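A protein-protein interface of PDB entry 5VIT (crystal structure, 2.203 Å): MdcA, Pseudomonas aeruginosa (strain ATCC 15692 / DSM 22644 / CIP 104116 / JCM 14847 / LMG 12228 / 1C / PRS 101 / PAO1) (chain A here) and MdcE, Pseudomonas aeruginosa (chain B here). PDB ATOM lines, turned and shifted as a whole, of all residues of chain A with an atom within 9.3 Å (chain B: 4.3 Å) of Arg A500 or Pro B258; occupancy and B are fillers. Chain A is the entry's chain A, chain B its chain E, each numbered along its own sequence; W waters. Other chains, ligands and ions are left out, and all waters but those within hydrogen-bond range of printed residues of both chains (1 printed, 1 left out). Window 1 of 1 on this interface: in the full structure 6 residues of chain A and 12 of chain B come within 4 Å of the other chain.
NH2 of Arg A500 is in hydrogen-bond range of O of Asp B253 (2.9 Å).
The backbone carbonyl oxygen of Ile B254 is in hydrogen-bond range of the guanidinium group of Arg A500 (3.2 Å).
The guanidinium group (NH2) of Arg A500 lies within hydrogen-bond range of the backbone carbonyl oxygen (O) of Leu B255 (2.6 Å).
NH2 of Arg A500 lies close to N of Gly B257, at 3.2 Å.
The side-chain carboxylate (OD2) of Asp A498 lies within salt-bridge range of the guanidinium group (NH1) of Arg A500 (2.9 Å).
Arg A500 touches Gly B256 (NH2 to C, 3.8 Å).
O of Arg A500 touches CG of Pro B258, at 3.6 Å.
Glu A501 touches Pro B258 (OE2 to CG, 3.6 Å).
Of chain B, only Asp B253 (2.9 Å), Ile B254 (3.2 Å), Leu B255 (2.6 Å), Gly B256 (3.8 Å), Gly B257 (3.2 Å) and Pro B258 (3.6 Å) come within 4 Å of Arg A500.
Of the printed residues of chain A, Pro B258 touches Arg A500 (3.6 Å) and Glu A501 (3.6 Å).
Of chain A, only Arg A500 (3.8 Å) comes within 4 Å of Gly B256.
Of chain A, only Arg A500 comes within 4 Å of Gly B257.
Of the printed residues of chain B, Glu A501 touches Pro B258 (3.6 Å).
Of the printed residues of chain A, Leu B255 touches Arg A500 (2.6 Å).
Of the printed residues of chain A, Asp B253 touches Arg A500.
The nearest printed residue of chain B that does not touch Arg A500 is Ala B252 (4.3 Å).
The nearest printed residue of chain A that does not touch Asp B253 is Pro A499 (6.9 Å).
Along chain A the printed residues that touch a printed residue of chain B span positions 500 to 501.
Hydrophobic or aromatic side chains of chain B that line the printed part of chain A: Pro B258.
Among the printed residues, no Asp or Glu carboxylate lies within 4 Å of a Lys or Arg side-chain nitrogen of the other chain.
Water W1 bridges the side-chain carboxylate (OD1) of Asp B260 (2.6 Å) and the side-chain amide oxygen (OE1) of Gln A503 (3.0 Å).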
ATOM      1  N   ARG A 496     -24.886  30.069  19.960  1.00  0.00           N
ATOM      2  CA  ARG A 496     -24.593  31.363  19.328  1.00  0.00           C
ATOM      3  C   ARG A 496     -23.389  31.291  18.386  1.00  0.00           C
ATOM      4  O   ARG A 496     -23.170  32.199  17.580  1.00  0.00           O
ATOM      5  CB  ARG A 496     -24.324  32.445  20.384  1.00  0.00           C
ATOM      6  CG  ARG A 496     -25.481  32.746  21.309  1.00  0.00           C
ATOM      7  CD  ARG A 496     -25.044  33.681  22.423  1.00  0.00           C
ATOM      8  NE  ARG A 496     -26.151  34.028  23.322  1.00  0.00           N
ATOM      9  CZ  ARG A 496     -26.045  34.836  24.379  1.00  0.00           C
ATOM     10  NH1 ARG A 496     -24.876  35.404  24.684  1.00  0.00           N
ATOM     11  NH2 ARG A 496     -27.115  35.085  25.129  1.00  0.00           N
ATOM     12  N   HIS A 497     -22.599  30.223  18.503  1.00  0.00           N
ATOM     13  CA  HIS A 497     -21.408  30.055  17.674  1.00  0.00           C
ATOM     14  C   HIS A 497     -21.694  29.530  16.271  1.00  0.00           C
ATOM     15  O   HIS A 497     -22.373  28.518  16.099  1.00  0.00           O
ATOM     16  CB  HIS A 497     -20.418  29.114  18.347  1.00  0.00           C
ATOM     17  CG  HIS A 497     -19.154  28.928  17.571  1.00  0.00           C
ATOM     18  ND1 HIS A 497     -18.266  29.961  17.338  1.00  0.00           N
ATOM     19  CD2 HIS A 497     -18.627  27.831  16.974  1.00  0.00           C
ATOM     20  CE1 HIS A 497     -17.241  29.503  16.639  1.00  0.00           C
ATOM     21  NE2 HIS A 497     -17.438  28.216  16.401  1.00  0.00           N
ATOM     22  N   ASP A 498     -21.156  30.236  15.279  1.00  0.00           N
ATOM     23  CA  ASP A 498     -21.154  29.804  13.881  1.00  0.00           C
ATOM     24  C   ASP A 498     -19.996  28.840  13.633  1.00  0.00           C
ATOM     25  O   ASP A 498     -18.822  29.240  13.650  1.00  0.00           O
ATOM     26  CB  ASP A 498     -21.043  31.012  12.951  1.00  0.00           C
ATOM     27  CG  ASP A 498     -21.143  30.635  11.465  1.00  0.00           C
ATOM     28  OD1 ASP A 498     -21.149  29.442  11.143  1.00  0.00           O
ATOM     29  OD2 ASP A 498     -21.220  31.549  10.616  1.00  0.00           O
ATOM     30  N   PRO A 499     -20.321  27.568  13.386  1.00  0.00           N
ATOM     31  CA  PRO A 499     -19.265  26.549  13.291  1.00  0.00           C
ATOM     32  C   PRO A 499     -18.257  26.819  12.166  1.00  0.00           C
ATOM     33  O   PRO A 499     -17.137  26.308  12.266  1.00  0.00           O
ATOM     34  CB  PRO A 499     -20.040  25.240  13.058  1.00  0.00           C
ATOM     35  CG  PRO A 499     -21.453  25.646  12.741  1.00  0.00           C
ATOM     36  CD  PRO A 499     -21.679  26.998  13.329  1.00  0.00           C
ATOM     37  N   ARG A 500     -18.602  27.620  11.154  1.00  0.00           N
ATOM     38  CA  ARG A 500     -17.625  27.935  10.109  1.00  0.00           C
ATOM     39  C   ARG A 500     -16.545  28.882  10.610  1.00  0.00           C
ATOM     40  O   ARG A 500     -15.593  29.175   9.881  1.00  0.00           O
ATOM     41  CB  ARG A 500     -18.270  28.577   8.886  1.00  0.00           C
ATOM     42  CG  ARG A 500     -19.470  27.870   8.324  1.00  0.00           C
ATOM     43  CD  ARG A 500     -20.569  28.878   8.396  1.00  0.00           C
ATOM     44  NE  ARG A 500     -21.188  29.194   7.148  1.00  0.00           N
ATOM     45  CZ  ARG A 500     -22.070  30.181   6.999  1.00  0.00           C
ATOM     46  NH1 ARG A 500     -22.395  30.945   8.028  1.00  0.00           N
ATOM     47  NH2 ARG A 500     -22.614  30.407   5.809  1.00  0.00           N
ATOM     48  N   GLU A 501     -16.723  29.390  11.831  1.00  0.00           N
ATOM     49  CA  GLU A 501     -15.732  30.264  12.459  1.00  0.00           C
ATOM     50  C   GLU A 501     -14.716  29.465  13.285  1.00  0.00           C
ATOM     51  O   GLU A 501     -13.665  29.985  13.664  1.00  0.00           O
ATOM     52  CB  GLU A 501     -16.419  31.318  13.348  1.00  0.00           C
ATOM     53  CG  GLU A 501     -17.259  32.357  12.597  1.00  0.00           C
ATOM     54  CD  GLU A 501     -16.460  33.124  11.539  1.00  0.00           C
ATOM     55  OE1 GLU A 501     -15.243  33.341  11.733  1.00  0.00           O
ATOM     56  OE2 GLU A 501     -17.052  33.511  10.508  1.00  0.00           O
ATOM     57  N   THR A 502     -15.027  28.206  13.568  1.00  0.00           N
ATOM     58  CA  THR A 502     -14.155  27.402  14.429  1.00  0.00           C
ATOM     59  C   THR A 502     -12.731  27.248  13.873  1.00  0.00           C
ATOM     60  O   THR A 502     -11.760  27.363  14.634  1.00  0.00           O
ATOM     61  CB  THR A 502     -14.753  26.003  14.682  1.00  0.00           C
ATOM     62  OG1 THR A 502     -15.989  26.148  15.369  1.00  0.00           O
ATOM     63  CG2 THR A 502     -13.813  25.133  15.544  1.00  0.00           C
ATOM     64  N   GLN A 503     -12.603  27.019  12.561  1.00  0.00           N
ATOM     65  CA  GLN A 503     -11.290  26.747  11.961  1.00  0.00           C
ATOM     66  C   GLN A 503     -10.317  27.909  12.183  1.00  0.00           C
ATOM     67  O   GLN A 503      -9.163  27.715  12.565  1.00  0.00           O
ATOM     68  CB  GLN A 503     -11.418  26.455  10.461  1.00  0.00           C
ATOM     69  CG  GLN A 503     -10.077  26.134   9.765  1.00  0.00           C
ATOM     70  CD  GLN A 503      -9.388  27.359   9.137  1.00  0.00           C
ATOM     71  OE1 GLN A 503     -10.038  28.369   8.793  1.00  0.00           O
ATOM     72  NE2 GLN A 503      -8.063  27.272   8.985  1.00  0.00           N
ATOM     73  N   ARG A 504     -10.803  29.115  11.944  1.00  0.00           N
ATOM     74  CA  ARG A 504     -10.027  30.319  12.165  1.00  0.00           C
ATOM     75  C   ARG A 504      -9.584  30.469  13.620  1.00  0.00           C
ATOM     76  O   ARG A 504      -8.431  30.825  13.894  1.00  0.00           O
ATOM     77  CB  ARG A 504     -10.848  31.535  11.741  1.00  0.00           C
ATOM     78  CG  ARG A 504     -10.221  32.883  12.058  1.00  0.00           C
ATOM     79  CD  ARG A 504     -10.653  33.877  11.007  1.00  0.00           C
ATOM     80  NE  ARG A 504      -9.611  34.861  10.772  1.00  0.00           N
ATOM     81  CZ  ARG A 504      -9.062  35.103   9.586  1.00  0.00           C
ATOM     82  NH1 ARG A 504      -9.450  34.424   8.507  1.00  0.00           N
ATOM     83  NH2 ARG A 504      -8.119  36.031   9.489  1.00  0.00           N
ATOM     84  N   MET A 505     -10.499  30.207  14.552  1.00  0.00           N
ATOM     85  CA  MET A 505     -10.173  30.343  15.964  1.00  0.00           C
ATOM     86  C   MET A 505      -9.122  29.314  16.358  1.00  0.00           C
ATOM     87  O   MET A 505      -8.218  29.608  17.144  1.00  0.00           O
ATOM     88  CB  MET A 505     -11.430  30.215  16.806  1.00  0.00           C
ATOM     89  CG  MET A 505     -12.450  31.307  16.444  1.00  0.00           C
ATOM     90  SD  MET A 505     -13.959  31.288  17.424  1.00  0.00           S
ATOM     91  CE  MET A 505     -13.347  31.903  18.983  1.00  0.00           C
ATOM     92  N   ARG A 506      -9.218  28.124  15.774  1.00  0.00           N
ATOM     93  CA  ARG A 506      -8.224  27.073  15.984  1.00  0.00           C
ATOM     94  C   ARG A 506      -6.829  27.487  15.503  1.00  0.00           C
ATOM     95  O   ARG A 506      -5.838  27.421  16.233  1.00  0.00           O
ATOM     96  CB  ARG A 506      -8.646  25.813  15.248  1.00  0.00           C
ATOM     97  CG  ARG A 506      -9.927  25.199  15.765  1.00  0.00           C
ATOM     98  CD  ARG A 506      -9.684  23.756  15.953  1.00  0.00           C
ATOM     99  NE  ARG A 506     -10.230  22.909  14.924  1.00  0.00           N
ATOM    100  CZ  ARG A 506      -9.744  21.711  14.617  1.00  0.00           C
ATOM    101  NH1 ARG A 506      -8.662  21.241  15.229  1.00  0.00           N
ATOM    102  NH2 ARG A 506     -10.332  20.992  13.674  1.00  0.00           N
ATOM    103  N   ARG A 507      -6.789  27.900  14.246  1.00  0.00           N
ATOM    104  CA  ARG A 507      -5.582  28.335  13.591  1.00  0.00           C
ATOM    105  C   ARG A 507      -4.918  29.530  14.293  1.00  0.00           C
ATOM    106  O   ARG A 507      -3.702  29.561  14.426  1.00  0.00           O
ATOM    107  CB  ARG A 507      -5.899  28.675  12.143  1.00  0.00           C
ATOM    108  CG  ARG A 507      -4.686  28.781  11.248  1.00  0.00           C
ATOM    109  CD  ARG A 507      -5.105  29.016   9.799  1.00  0.00           C
ATOM    110  NE  ARG A 507      -6.239  29.940   9.663  1.00  0.00           N
ATOM    111  CZ  ARG A 507      -6.084  31.264   9.807  1.00  0.00           C
ATOM    112  NH1 ARG A 507      -4.853  31.766  10.068  1.00  0.00           N
ATOM    113  NH2 ARG A 507      -7.123  32.114   9.682  1.00  0.00           N
ATOM    114  N   ALA B 252     -26.725  27.102   0.595  1.00  0.00           N
ATOM    115  CA  ALA B 252     -27.131  27.680   1.877  1.00  0.00           C
ATOM    116  C   ALA B 252     -25.975  27.677   2.875  1.00  0.00           C
ATOM    117  O   ALA B 252     -25.799  28.620   3.635  1.00  0.00           O
ATOM    118  CB  ALA B 252     -28.336  26.911   2.459  1.00  0.00           C
ATOM    119  N   ASP B 253     -25.181  26.612   2.862  1.00  0.00           N
ATOM    120  CA  ASP B 253     -24.080  26.483   3.813  1.00  0.00           C
ATOM    121  C   ASP B 253     -22.956  27.480   3.537  1.00  0.00           C
ATOM    122  O   ASP B 253     -22.214  27.876   4.452  1.00  0.00           O
ATOM    123  CB  ASP B 253     -23.524  25.069   3.793  1.00  0.00           C
ATOM    124  CG  ASP B 253     -22.506  24.840   4.902  1.00  0.00           C
ATOM    125  OD1 ASP B 253     -22.927  24.742   6.075  1.00  0.00           O
ATOM    126  OD2 ASP B 253     -21.295  24.769   4.601  1.00  0.00           O
ATOM    127  N   ILE B 254     -22.849  27.893   2.277  1.00  0.00           N
ATOM    128  CA  ILE B 254     -21.851  28.879   1.861  1.00  0.00           C
ATOM    129  C   ILE B 254     -22.241  30.311   2.224  1.00  0.00           C
ATOM    130  O   ILE B 254     -21.478  31.023   2.893  1.00  0.00           O
ATOM    131  CB  ILE B 254     -21.604  28.805   0.345  1.00  0.00           C
ATOM    132  CG1 ILE B 254     -20.958  27.463  -0.003  1.00  0.00           C
ATOM    133  CG2 ILE B 254     -20.740  29.982  -0.126  1.00  0.00           C
ATOM    134  CD1 ILE B 254     -20.946  27.125  -1.476  1.00  0.00           C
ATOM    135  N   LEU B 255     -23.425  30.722   1.779  1.00  0.00           N
ATOM    136  CA  LEU B 255     -23.856  32.116   1.870  1.00  0.00           C
ATOM    137  C   LEU B 255     -23.666  32.705   3.264  1.00  0.00           C
ATOM    138  O   LEU B 255     -23.968  32.068   4.269  1.00  0.00           O
ATOM    139  CB  LEU B 255     -25.321  32.225   1.436  1.00  0.00           C
ATOM    140  CG  LEU B 255     -25.483  32.007  -0.078  1.00  0.00           C
ATOM    141  CD1 LEU B 255     -26.932  31.794  -0.535  1.00  0.00           C
ATOM    142  CD2 LEU B 255     -24.858  33.189  -0.807  1.00  0.00           C
ATOM    143  N   GLY B 256     -23.131  33.913   3.317  1.00  0.00           N
ATOM    144  CA  GLY B 256     -22.970  34.590   4.585  1.00  0.00           C
ATOM    145  C   GLY B 256     -21.808  34.110   5.443  1.00  0.00           C
ATOM    146  O   GLY B 256     -21.554  34.682   6.492  1.00  0.00           O
ATOM    147  N   GLY B 257     -21.103  33.067   5.012  1.00  0.00           N
ATOM    148  CA  GLY B 257     -19.986  32.551   5.787  1.00  0.00           C
ATOM    149  C   GLY B 257     -18.661  32.969   5.189  1.00  0.00           C
ATOM    150  O   GLY B 257     -18.634  33.740   4.235  1.00  0.00           O
ATOM    151  N   PRO B 258     -17.555  32.474   5.760  1.00  0.00           N
ATOM    152  CA  PRO B 258     -16.211  32.724   5.229  1.00  0.00           C
ATOM    153  C   PRO B 258     -16.082  32.242   3.794  1.00  0.00           C
ATOM    154  O   PRO B 258     -16.610  31.183   3.450  1.00  0.00           O
ATOM    155  CB  PRO B 258     -15.302  31.903   6.159  1.00  0.00           C
ATOM    156  CG  PRO B 258     -16.082  31.805   7.450  1.00  0.00           C
ATOM    157  CD  PRO B 258     -17.523  31.689   7.009  1.00  0.00           C
ATOM    158  N   ARG B 259     -15.370  33.008   2.977  1.00  0.00           N
ATOM    159  CA  ARG B 259     -15.254  32.727   1.545  1.00  0.00           C
ATOM    160  C   ARG B 259     -14.000  31.931   1.211  1.00  0.00           C
ATOM    161  O   ARG B 259     -13.765  31.587   0.050  1.00  0.00           O
ATOM    162  CB  ARG B 259     -15.269  34.043   0.756  1.00  0.00           C
ATOM    163  CG  ARG B 259     -16.565  34.836   0.962  1.00  0.00           C
ATOM    164  CD  ARG B 259     -16.614  36.111   0.135  1.00  0.00           C
ATOM    165  NE  ARG B 259     -17.781  36.918   0.485  1.00  0.00           N
ATOM    166  CZ  ARG B 259     -17.964  38.175   0.086  1.00  0.00           C
ATOM    167  NH1 ARG B 259     -17.060  38.772  -0.679  1.00  0.00           N
ATOM    168  NH2 ARG B 259     -19.051  38.836   0.450  1.00  0.00           N
ATOM    169  N   ASP B 260     -13.182  31.647   2.222  1.00  0.00           N
ATOM    170  CA  ASP B 260     -11.943  30.938   1.971  1.00  0.00           C
ATOM    171  C   ASP B 260     -12.154  29.439   1.944  1.00  0.00           C
ATOM    172  O   ASP B 260     -13.278  28.946   1.889  1.00  0.00           O
ATOM    173  CB  ASP B 260     -10.880  31.292   3.009  1.00  0.00           C
ATOM    174  CG  ASP B 260     -11.355  31.071   4.427  1.00  0.00           C
ATOM    175  OD1 ASP B 260     -11.844  29.961   4.749  1.00  0.00           O
ATOM    176  OD2 ASP B 260     -11.255  32.021   5.220  1.00  0.00           O
HETATM  177  O   HOH W   1     -12.353  29.283   7.189  1.00  0.00           O
